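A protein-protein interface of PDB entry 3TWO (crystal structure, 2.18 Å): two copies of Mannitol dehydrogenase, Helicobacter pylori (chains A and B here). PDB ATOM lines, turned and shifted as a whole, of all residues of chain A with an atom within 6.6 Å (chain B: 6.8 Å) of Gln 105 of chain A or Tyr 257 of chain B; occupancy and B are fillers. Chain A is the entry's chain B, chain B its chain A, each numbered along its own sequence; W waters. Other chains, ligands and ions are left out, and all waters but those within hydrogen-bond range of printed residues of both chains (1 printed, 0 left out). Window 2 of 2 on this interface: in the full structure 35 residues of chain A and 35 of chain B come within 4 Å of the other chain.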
ATOM      1  N   PHE A  91     -14.829  -2.843 -23.066  1.00  0.00           N
ATOM      2  CA  PHE A  91     -15.643  -1.841 -23.774  1.00  0.00           C
ATOM      3  C   PHE A  91     -14.854  -0.560 -24.011  1.00  0.00           C
ATOM      4  O   PHE A  91     -13.908  -0.282 -23.272  1.00  0.00           O
ATOM      5  CB  PHE A  91     -16.983  -1.550 -23.071  1.00  0.00           C
ATOM      6  CG  PHE A  91     -16.812  -1.210 -21.619  1.00  0.00           C
ATOM      7  CD1 PHE A  91     -16.567   0.094 -21.224  1.00  0.00           C
ATOM      8  CD2 PHE A  91     -16.868  -2.210 -20.646  1.00  0.00           C
ATOM      9  CE1 PHE A  91     -16.387   0.413 -19.872  1.00  0.00           C
ATOM     10  CE2 PHE A  91     -16.719  -1.900 -19.309  1.00  0.00           C
ATOM     11  CZ  PHE A  91     -16.466  -0.576 -18.928  1.00  0.00           C
ATOM     12  N   CYS A  98     -26.267   8.069 -18.260  1.00  0.00           N
ATOM     13  CA  CYS A  98     -27.226   7.241 -17.544  1.00  0.00           C
ATOM     14  C   CYS A  98     -26.754   6.831 -16.121  1.00  0.00           C
ATOM     15  O   CYS A  98     -25.638   7.158 -15.666  1.00  0.00           O
ATOM     16  CB  CYS A  98     -27.542   5.984 -18.378  1.00  0.00           C
ATOM     17  SG  CYS A  98     -26.080   4.785 -18.369  1.00  0.00           S
ATOM     18  N   LYS A  99     -27.623   6.126 -15.416  1.00  0.00           N
ATOM     19  CA  LYS A  99     -27.338   5.807 -14.044  1.00  0.00           C
ATOM     20  C   LYS A  99     -26.132   4.907 -13.994  1.00  0.00           C
ATOM     21  O   LYS A  99     -25.234   5.206 -13.270  1.00  0.00           O
ATOM     22  CB  LYS A  99     -28.517   5.133 -13.334  1.00  0.00           C
ATOM     23  CG  LYS A  99     -28.354   5.153 -11.805  1.00  0.00           C
ATOM     24  CD  LYS A  99     -29.680   5.421 -11.096  1.00  0.00           C
ATOM     25  CE  LYS A  99     -30.642   4.193 -11.121  1.00  0.00           C
ATOM     26  NZ  LYS A  99     -29.962   3.026 -10.472  1.00  0.00           N
ATOM     27  N   PRO A 100     -26.109   3.819 -14.782  1.00  0.00           N
ATOM     28  CA  PRO A 100     -24.879   3.025 -14.679  1.00  0.00           C
ATOM     29  C   PRO A 100     -23.589   3.813 -15.040  1.00  0.00           C
ATOM     30  O   PRO A 100     -22.573   3.605 -14.363  1.00  0.00           O
ATOM     31  CB  PRO A 100     -25.128   1.860 -15.637  1.00  0.00           C
ATOM     32  CG  PRO A 100     -26.585   1.708 -15.681  1.00  0.00           C
ATOM     33  CD  PRO A 100     -27.210   3.047 -15.398  1.00  0.00           C
ATOM     34  N   CYS A 101     -23.619   4.666 -16.072  1.00  0.00           N
ATOM     35  CA  CYS A 101     -22.447   5.428 -16.441  1.00  0.00           C
ATOM     36  C   CYS A 101     -22.032   6.329 -15.307  1.00  0.00           C
ATOM     37  O   CYS A 101     -20.815   6.445 -15.048  1.00  0.00           O
ATOM     38  CB  CYS A 101     -22.643   6.274 -17.712  1.00  0.00           C
ATOM     39  SG  CYS A 101     -22.552   5.296 -19.254  1.00  0.00           S
ATOM     40  N   LYS A 102     -23.015   6.965 -14.649  1.00  0.00           N
ATOM     41  CA  LYS A 102     -22.715   7.881 -13.546  1.00  0.00           C
ATOM     42  C   LYS A 102     -22.181   7.123 -12.309  1.00  0.00           C
ATOM     43  O   LYS A 102     -21.323   7.635 -11.603  1.00  0.00           O
ATOM     44  CB  LYS A 102     -23.919   8.735 -13.189  1.00  0.00           C
ATOM     45  CG  LYS A 102     -23.967  10.093 -13.991  1.00  0.00           C
ATOM     46  CD  LYS A 102     -23.564  10.006 -15.512  1.00  0.00           C
ATOM     47  CE  LYS A 102     -24.046  11.242 -16.239  1.00  0.00           C
ATOM     48  NZ  LYS A 102     -23.856  12.468 -15.429  1.00  0.00           N
ATOM     49  N   GLU A 103     -22.642   5.890 -12.087  1.00  0.00           N
ATOM     50  CA  GLU A 103     -22.115   5.070 -11.000  1.00  0.00           C
ATOM     51  C   GLU A 103     -20.829   4.289 -11.389  1.00  0.00           C
ATOM     52  O   GLU A 103     -20.421   3.351 -10.685  1.00  0.00           O
ATOM     53  CB  GLU A 103     -23.226   4.171 -10.437  1.00  0.00           C
ATOM     54  CG  GLU A 103     -24.236   5.065  -9.736  1.00  0.00           C
ATOM     55  CD  GLU A 103     -25.509   4.357  -9.314  1.00  0.00           C
ATOM     56  OE1 GLU A 103     -25.786   3.229  -9.782  1.00  0.00           O
ATOM     57  OE2 GLU A 103     -26.251   4.937  -8.488  1.00  0.00           O
ATOM     58  N   HIS A 104     -20.171   4.677 -12.486  1.00  0.00           N
ATOM     59  CA  HIS A 104     -18.929   3.992 -12.861  1.00  0.00           C
ATOM     60  C   HIS A 104     -19.133   2.478 -13.090  1.00  0.00           C
ATOM     61  O   HIS A 104     -18.263   1.661 -12.756  1.00  0.00           O
ATOM     62  CB  HIS A 104     -17.896   4.152 -11.740  1.00  0.00           C
ATOM     63  CG  HIS A 104     -17.649   5.556 -11.373  1.00  0.00           C
ATOM     64  ND1 HIS A 104     -17.003   6.437 -12.220  1.00  0.00           N
ATOM     65  CD2 HIS A 104     -17.969   6.255 -10.254  1.00  0.00           C
ATOM     66  CE1 HIS A 104     -16.932   7.618 -11.631  1.00  0.00           C
ATOM     67  NE2 HIS A 104     -17.517   7.534 -10.449  1.00  0.00           N
ATOM     68  N   GLN A 105     -20.285   2.127 -13.652  1.00  0.00           N
ATOM     69  CA  GLN A 105     -20.538   0.762 -14.104  1.00  0.00           C
ATOM     70  C   GLN A 105     -20.967   0.842 -15.586  1.00  0.00           C
ATOM     71  O   GLN A 105     -22.077   0.392 -15.955  1.00  0.00           O
ATOM     72  CB  GLN A 105     -21.695   0.164 -13.305  1.00  0.00           C
ATOM     73  CG  GLN A 105     -21.541   0.161 -11.843  1.00  0.00           C
ATOM     74  CD  GLN A 105     -21.010  -1.158 -11.409  1.00  0.00           C
ATOM     75  OE1 GLN A 105     -19.793  -1.377 -11.476  1.00  0.00           O
ATOM     76  NE2 GLN A 105     -21.916  -2.091 -10.987  1.00  0.00           N
ATOM     77  N   GLU A 106     -20.094   1.410 -16.416  1.00  0.00           N
ATOM     78  CA  GLU A 106     -20.396   1.634 -17.825  1.00  0.00           C
ATOM     79  C   GLU A 106     -20.737   0.315 -18.543  1.00  0.00           C
ATOM     80  O   GLU A 106     -21.422   0.341 -19.561  1.00  0.00           O
ATOM     81  CB  GLU A 106     -19.236   2.388 -18.547  1.00  0.00           C
ATOM     82  CG  GLU A 106     -18.783   3.662 -17.823  1.00  0.00           C
ATOM     83  CD  GLU A 106     -17.603   3.412 -16.843  1.00  0.00           C
ATOM     84  OE1 GLU A 106     -17.353   2.242 -16.411  1.00  0.00           O
ATOM     85  OE2 GLU A 106     -16.901   4.401 -16.535  1.00  0.00           O
ATOM     86  N   GLN A 107     -20.349  -0.821 -17.969  1.00  0.00           N
ATOM     87  CA  GLN A 107     -20.618  -2.129 -18.617  1.00  0.00           C
ATOM     88  C   GLN A 107     -22.087  -2.448 -18.681  1.00  0.00           C
ATOM     89  O   GLN A 107     -22.442  -3.289 -19.449  1.00  0.00           O
ATOM     90  CB  GLN A 107     -19.885  -3.333 -17.956  1.00  0.00           C
ATOM     91  CG  GLN A 107     -20.445  -3.776 -16.551  1.00  0.00           C
ATOM     92  CD  GLN A 107     -19.827  -3.008 -15.400  1.00  0.00           C
ATOM     93  OE1 GLN A 107     -19.400  -1.860 -15.569  1.00  0.00           O
ATOM     94  NE2 GLN A 107     -19.743  -3.653 -14.216  1.00  0.00           N
ATOM     95  N   PHE A 108     -22.924  -1.779 -17.886  1.00  0.00           N
ATOM     96  CA  PHE A 108     -24.358  -1.962 -17.929  1.00  0.00           C
ATOM     97  C   PHE A 108     -25.072  -0.850 -18.695  1.00  0.00           C
ATOM     98  O   PHE A 108     -26.284  -0.872 -18.790  1.00  0.00           O
ATOM     99  CB  PHE A 108     -24.966  -2.088 -16.506  1.00  0.00           C
ATOM    100  CG  PHE A 108     -24.465  -3.269 -15.746  1.00  0.00           C
ATOM    101  CD1 PHE A 108     -23.638  -3.096 -14.639  1.00  0.00           C
ATOM    102  CD2 PHE A 108     -24.826  -4.540 -16.136  1.00  0.00           C
ATOM    103  CE1 PHE A 108     -23.146  -4.206 -13.922  1.00  0.00           C
ATOM    104  CE2 PHE A 108     -24.333  -5.690 -15.433  1.00  0.00           C
ATOM    105  CZ  PHE A 108     -23.475  -5.504 -14.327  1.00  0.00           C
ATOM    106  N   CYS A 109     -24.336   0.130 -19.227  1.00  0.00           N
ATOM    107  CA  CYS A 109     -24.948   1.136 -20.072  1.00  0.00           C
ATOM    108  C   CYS A 109     -25.652   0.453 -21.262  1.00  0.00           C
ATOM    109  O   CYS A 109     -25.089  -0.410 -21.929  1.00  0.00           O
ATOM    110  CB  CYS A 109     -23.919   2.129 -20.617  1.00  0.00           C
ATOM    111  SG  CYS A 109     -24.647   3.410 -21.699  1.00  0.00           S
ATOM    112  N   SER A 167     -13.487  -7.880  -9.060  1.00  0.00           N
ATOM    113  CA  SER A 167     -14.675  -7.104  -8.700  1.00  0.00           C
ATOM    114  C   SER A 167     -15.578  -7.845  -7.666  1.00  0.00           C
ATOM    115  O   SER A 167     -15.952  -7.273  -6.696  1.00  0.00           O
ATOM    116  CB  SER A 167     -15.466  -6.646  -9.960  1.00  0.00           C
ATOM    117  OG  SER A 167     -16.616  -5.821  -9.596  1.00  0.00           O
ATOM    118  N   LYS A 170     -14.147  -8.155  -4.078  1.00  0.00           N
ATOM    119  CA  LYS A 170     -14.342  -6.934  -3.309  1.00  0.00           C
ATOM    120  C   LYS A 170     -15.796  -6.719  -2.970  1.00  0.00           C
ATOM    121  O   LYS A 170     -16.093  -6.350  -1.872  1.00  0.00           O
ATOM    122  CB  LYS A 170     -13.917  -5.670  -4.101  1.00  0.00           C
ATOM    123  CG  LYS A 170     -12.577  -5.810  -4.790  1.00  0.00           C
ATOM    124  CD  LYS A 170     -11.514  -5.163  -4.000  1.00  0.00           C
ATOM    125  CE  LYS A 170     -11.338  -5.634  -2.646  1.00  0.00           C
ATOM    126  NZ  LYS A 170     -11.051  -4.255  -1.974  1.00  0.00           N
ATOM    127  N   PHE A 171     -16.689  -6.904  -3.930  1.00  0.00           N
ATOM    128  CA  PHE A 171     -18.116  -6.737  -3.669  1.00  0.00           C
ATOM    129  C   PHE A 171     -18.630  -7.624  -2.503  1.00  0.00           C
ATOM    130  O   PHE A 171     -19.367  -7.136  -1.660  1.00  0.00           O
ATOM    131  CB  PHE A 171     -18.915  -7.052  -4.945  1.00  0.00           C
ATOM    132  CG  PHE A 171     -20.409  -7.017  -4.783  1.00  0.00           C
ATOM    133  CD1 PHE A 171     -21.104  -5.806  -4.602  1.00  0.00           C
ATOM    134  CD2 PHE A 171     -21.153  -8.204  -4.888  1.00  0.00           C
ATOM    135  CE1 PHE A 171     -22.542  -5.795  -4.526  1.00  0.00           C
ATOM    136  CE2 PHE A 171     -22.557  -8.186  -4.801  1.00  0.00           C
ATOM    137  CZ  PHE A 171     -23.256  -6.966  -4.630  1.00  0.00           C
ATOM    138  N   LEU A 292     -20.475  -8.740 -14.105  1.00  0.00           N
ATOM    139  CA  LEU A 292     -20.091  -8.465 -15.456  1.00  0.00           C
ATOM    140  C   LEU A 292     -18.877  -7.525 -15.415  1.00  0.00           C
ATOM    141  O   LEU A 292     -19.004  -6.333 -15.055  1.00  0.00           O
ATOM    142  CB  LEU A 292     -21.246  -7.803 -16.228  1.00  0.00           C
ATOM    143  CG  LEU A 292     -20.946  -7.504 -17.721  1.00  0.00           C
ATOM    144  CD1 LEU A 292     -20.583  -8.735 -18.510  1.00  0.00           C
ATOM    145  CD2 LEU A 292     -22.157  -6.773 -18.306  1.00  0.00           C
ATOM    146  N   GLY A 294     -16.181  -5.003 -15.080  1.00  0.00           N
ATOM    147  CA  GLY A 294     -16.172  -3.966 -14.049  1.00  0.00           C
ATOM    148  C   GLY A 294     -16.188  -2.648 -14.771  1.00  0.00           C
ATOM    149  O   GLY A 294     -15.960  -2.592 -15.978  1.00  0.00           O
ATOM    150  N   GLY A 295     -16.445  -1.599 -14.040  1.00  0.00           N
ATOM    151  CA  GLY A 295     -16.335  -0.239 -14.554  1.00  0.00           C
ATOM    152  C   GLY A 295     -14.919   0.231 -14.784  1.00  0.00           C
ATOM    153  O   GLY A 295     -13.981  -0.405 -14.353  1.00  0.00           O
ATOM    154  N   ILE A 296     -14.774   1.347 -15.514  1.00  0.00           N
ATOM    155  CA  ILE A 296     -13.448   1.933 -15.778  1.00  0.00           C
ATOM    156  C   ILE A 296     -12.667   2.260 -14.479  1.00  0.00           C
ATOM    157  O   ILE A 296     -11.486   1.864 -14.280  1.00  0.00           O
ATOM    158  CB  ILE A 296     -13.591   3.168 -16.679  1.00  0.00           C
ATOM    159  CG1 ILE A 296     -14.069   2.717 -18.078  1.00  0.00           C
ATOM    160  CG2 ILE A 296     -12.280   3.966 -16.727  1.00  0.00           C
ATOM    161  CD1 ILE A 296     -13.104   1.625 -18.805  1.00  0.00           C
ATOM    162  N   GLU A 298     -13.044   1.006 -11.448  1.00  0.00           N
ATOM    163  CA  GLU A 298     -12.606  -0.100 -10.617  1.00  0.00           C
ATOM    164  C   GLU A 298     -11.527  -0.857 -11.407  1.00  0.00           C
ATOM    165  O   GLU A 298     -10.640  -1.493 -10.802  1.00  0.00           O
ATOM    166  CB  GLU A 298     -13.785  -1.030 -10.167  1.00  0.00           C
ATOM    167  CG  GLU A 298     -13.345  -2.057  -9.115  1.00  0.00           C
ATOM    168  CD  GLU A 298     -14.409  -3.072  -8.701  1.00  0.00           C
ATOM    169  OE1 GLU A 298     -15.392  -3.361  -9.471  1.00  0.00           O
ATOM    170  OE2 GLU A 298     -14.261  -3.643  -7.587  1.00  0.00           O
ATOM    171  N   GLU B 234     -35.137   2.178  -7.332  1.00  0.00           N
ATOM    172  CA  GLU B 234     -34.473   0.979  -6.912  1.00  0.00           C
ATOM    173  C   GLU B 234     -34.875   0.573  -5.535  1.00  0.00           C
ATOM    174  O   GLU B 234     -35.069   1.423  -4.686  1.00  0.00           O
ATOM    175  CB  GLU B 234     -32.969   1.198  -6.951  1.00  0.00           C
ATOM    176  CG  GLU B 234     -32.403   1.243  -8.384  1.00  0.00           C
ATOM    177  CD  GLU B 234     -30.882   1.338  -8.386  1.00  0.00           C
ATOM    178  OE1 GLU B 234     -30.248   0.792  -9.307  1.00  0.00           O
ATOM    179  OE2 GLU B 234     -30.315   1.970  -7.468  1.00  0.00           O
ATOM    180  N   LEU B 235     -34.957  -0.737  -5.293  1.00  0.00           N
ATOM    181  CA  LEU B 235     -35.399  -1.247  -4.001  1.00  0.00           C
ATOM    182  C   LEU B 235     -34.246  -1.958  -3.337  1.00  0.00           C
ATOM    183  O   LEU B 235     -33.432  -2.574  -3.992  1.00  0.00           O
ATOM    184  CB  LEU B 235     -36.589  -2.216  -4.208  1.00  0.00           C
ATOM    185  CG  LEU B 235     -37.831  -1.595  -4.889  1.00  0.00           C
ATOM    186  CD1 LEU B 235     -39.040  -2.551  -4.915  1.00  0.00           C
ATOM    187  CD2 LEU B 235     -38.263  -0.284  -4.216  1.00  0.00           C
ATOM    188  N   ASP B 236     -34.182  -1.871  -2.018  1.00  0.00           N
ATOM    189  CA  ASP B 236     -33.163  -2.568  -1.281  1.00  0.00           C
ATOM    190  C   ASP B 236     -33.510  -4.064  -1.130  1.00  0.00           C
ATOM    191  O   ASP B 236     -32.617  -4.893  -1.042  1.00  0.00           O
ATOM    192  CB  ASP B 236     -33.041  -1.928   0.084  1.00  0.00           C
ATOM    193  CG  ASP B 236     -32.717  -0.474  -0.006  1.00  0.00           C
ATOM    194  OD1 ASP B 236     -31.769  -0.177  -0.752  1.00  0.00           O
ATOM    195  OD2 ASP B 236     -33.429   0.368   0.610  1.00  0.00           O
ATOM    196  N   LEU B 255     -33.856  -4.158  -8.159  1.00  0.00           N
ATOM    197  CA  LEU B 255     -33.019  -4.077  -6.949  1.00  0.00           C
ATOM    198  C   LEU B 255     -31.910  -3.066  -7.173  1.00  0.00           C
ATOM    199  O   LEU B 255     -31.345  -2.963  -8.263  1.00  0.00           O
ATOM    200  CB  LEU B 255     -32.404  -5.441  -6.591  1.00  0.00           C
ATOM    201  CG  LEU B 255     -33.344  -6.515  -6.050  1.00  0.00           C
ATOM    202  CD1 LEU B 255     -32.530  -7.763  -5.731  1.00  0.00           C
ATOM    203  CD2 LEU B 255     -34.063  -5.953  -4.817  1.00  0.00           C
ATOM    204  N   THR B 256     -31.606  -2.312  -6.136  1.00  0.00           N
ATOM    205  CA  THR B 256     -30.424  -1.467  -6.210  1.00  0.00           C
ATOM    206  C   THR B 256     -29.159  -2.407  -6.209  1.00  0.00           C
ATOM    207  O   THR B 256     -29.257  -3.631  -6.008  1.00  0.00           O
ATOM    208  CB  THR B 256     -30.369  -0.519  -4.981  1.00  0.00           C
ATOM    209  OG1 THR B 256     -29.270   0.410  -5.180  1.00  0.00           O
ATOM    210  CG2 THR B 256     -30.149  -1.347  -3.677  1.00  0.00           C
ATOM    211  N   TYR B 257     -27.997  -1.837  -6.439  1.00  0.00           N
ATOM    212  CA  TYR B 257     -26.743  -2.551  -6.273  1.00  0.00           C
ATOM    213  C   TYR B 257     -26.593  -3.105  -4.835  1.00  0.00           C
ATOM    214  O   TYR B 257     -26.834  -2.407  -3.866  1.00  0.00           O
ATOM    215  CB  TYR B 257     -25.651  -1.570  -6.593  1.00  0.00           C
ATOM    216  CG  TYR B 257     -24.215  -2.014  -6.302  1.00  0.00           C
ATOM    217  CD1 TYR B 257     -23.370  -2.446  -7.371  1.00  0.00           C
ATOM    218  CD2 TYR B 257     -23.665  -1.891  -4.996  1.00  0.00           C
ATOM    219  CE1 TYR B 257     -21.991  -2.805  -7.123  1.00  0.00           C
ATOM    220  CE2 TYR B 257     -22.320  -2.214  -4.746  1.00  0.00           C
ATOM    221  CZ  TYR B 257     -21.484  -2.654  -5.834  1.00  0.00           C
ATOM    222  OH  TYR B 257     -20.165  -2.938  -5.610  1.00  0.00           O
ATOM    223  N   ASN B 258     -26.226  -4.361  -4.709  1.00  0.00           N
ATOM    224  CA  ASN B 258     -26.173  -5.022  -3.418  1.00  0.00           C
ATOM    225  C   ASN B 258     -27.558  -5.289  -2.784  1.00  0.00           C
ATOM    226  O   ASN B 258     -27.636  -5.566  -1.561  1.00  0.00           O
ATOM    227  CB  ASN B 258     -25.240  -4.319  -2.407  1.00  0.00           C
ATOM    228  CG  ASN B 258     -24.686  -5.276  -1.428  1.00  0.00           C
ATOM    229  OD1 ASN B 258     -24.349  -6.394  -1.800  1.00  0.00           O
ATOM    230  ND2 ASN B 258     -24.687  -4.918  -0.158  1.00  0.00           N
ATOM    231  N   GLY B 259     -28.626  -5.209  -3.598  1.00  0.00           N
ATOM    232  CA  GLY B 259     -29.961  -5.456  -3.076  1.00  0.00           C
ATOM    233  C   GLY B 259     -30.255  -6.952  -2.953  1.00  0.00           C
ATOM    234  O   GLY B 259     -29.537  -7.782  -3.563  1.00  0.00           O
ATOM    235  N   GLY B 284     -26.263  -7.660 -12.964  1.00  0.00           N
ATOM    236  CA  GLY B 284     -25.249  -7.973 -11.967  1.00  0.00           C
ATOM    237  C   GLY B 284     -25.376  -7.296 -10.610  1.00  0.00           C
ATOM    238  O   GLY B 284     -26.063  -6.287 -10.461  1.00  0.00           O
ATOM    239  N   ASN B 285     -24.711  -7.875  -9.616  1.00  0.00           N
ATOM    240  CA  ASN B 285     -24.607  -7.263  -8.257  1.00  0.00           C
ATOM    241  C   ASN B 285     -25.915  -7.186  -7.477  1.00  0.00           C
ATOM    242  O   ASN B 285     -26.069  -6.316  -6.606  1.00  0.00           O
ATOM    243  CB  ASN B 285     -23.908  -5.863  -8.325  1.00  0.00           C
ATOM    244  CG  ASN B 285     -22.501  -5.990  -8.805  1.00  0.00           C
ATOM    245  OD1 ASN B 285     -21.605  -6.487  -8.091  1.00  0.00           O
ATOM    246  ND2 ASN B 285     -22.282  -5.608 -10.004  1.00  0.00           N
ATOM    247  N   ARG B 286     -26.851  -8.077  -7.794  1.00  0.00           N
ATOM    248  CA  ARG B 286     -28.142  -8.088  -7.137  1.00  0.00           C
ATOM    249  C   ARG B 286     -28.359  -9.536  -6.709  1.00  0.00           C
ATOM    250  O   ARG B 286     -28.317 -10.475  -7.536  1.00  0.00           O
ATOM    251  CB  ARG B 286     -29.204  -7.655  -8.114  1.00  0.00           C
ATOM    252  CG  ARG B 286     -28.899  -6.236  -8.723  1.00  0.00           C
ATOM    253  CD  ARG B 286     -29.913  -6.007  -9.854  1.00  0.00           C
ATOM    254  NE  ARG B 286     -29.971  -4.671 -10.405  1.00  0.00           N
ATOM    255  CZ  ARG B 286     -29.323  -4.291 -11.527  1.00  0.00           C
ATOM    256  NH1 ARG B 286     -28.488  -5.131 -12.153  1.00  0.00           N
ATOM    257  NH2 ARG B 286     -29.479  -3.053 -12.024  1.00  0.00           N
HETATM  258  O   HOH W   1     -18.656  -7.374  -8.777  1.00  0.00           O
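OE1 of Glu 234 of chain B is in salt-bridge range of NZ of Lys 99 of chain A, at 2.5 Å.
OG1 of Thr 256 of chain B sits at hydrogen-bond distance from OE2 of Glu 234 of chain B. N of Asn 258 of chain B sits at hydrogen-bond distance from O of Asn 285 of chain B. The guanidinium group (NH1) of Arg 286 of chain B sits at hydrogen-bond distance from the backbone carbonyl oxygen (O) of Gly 284 of chain B. The backbone carbonyl oxygen (O) of Pro 100 of chain A lies within hydrogen-bond range of the backbone NH (N) of Gln 105 of chain A, at 2.8 Å.
Among the printed residues, merely in contact across the chains: Phe 171 of chain A with Asn 258 of chain B (3.1 Å), Phe 171 of chain A with Tyr 257 of chain B (3.2 Å), Phe 171 of chain A with Asn 285 of chain B (3.5 Å), Gln 105 of chain A with Asn 285 of chain B (3.7 Å), Phe 108 of chain A with Gly 284 of chain B (3.7 Å) and Gln 105 of chain A with Tyr 257 of chain B (3.9 Å).
Gln 105 of chain A touches just these residues of chain B: Tyr 257 (3.9 Å) and Asn 285 (3.7 Å). Of chain A, only Gln 105 (3.9 Å) and Phe 171 (3.2 Å) come within 4 Å of Tyr 257 of chain B. Printed residues of chain B within 4 Å of Phe 108 of chain A: Gly 284 (3.7 Å). Of the printed residues of chain A, Asn 258 of chain B touches Phe 171. Printed residues of chain A within 4 Å of Asn 285 of chain B: Gln 105 and Phe 171. Of the printed residues of chain A, Glu 234 of chain B touches Lys 99 (2.5 Å). Of the printed residues of chain A, Gly 284 of chain B touches Phe 108. Thr 256 of chain B touches none of the printed residues of chain A. Leu 292 of chain A touches none of the printed residues of chain B. The nearest residue of chain B that does not touch Gln 105 of chain A is Gly 284 of chain B (5.9 Å).
Of the 21 printed residues of chain A, 4 touch a printed residue of chain B. Hydrophobic or aromatic side chains of chain A that line the printed part of chain B: Phe 108 and Phe 171. Among the printed residues, 7 pairs touch across the chains.
No position is printed for both chains. Of the 7 pairs that touch across the chains among the printed residues, none has its exchanged pair printed and touching as well.
Water W1 lies within hydrogen-bond range of the side-chain hydroxyl of Ser 167 of chain A and the side-chain amide oxygen of Asn 285 of chain B.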
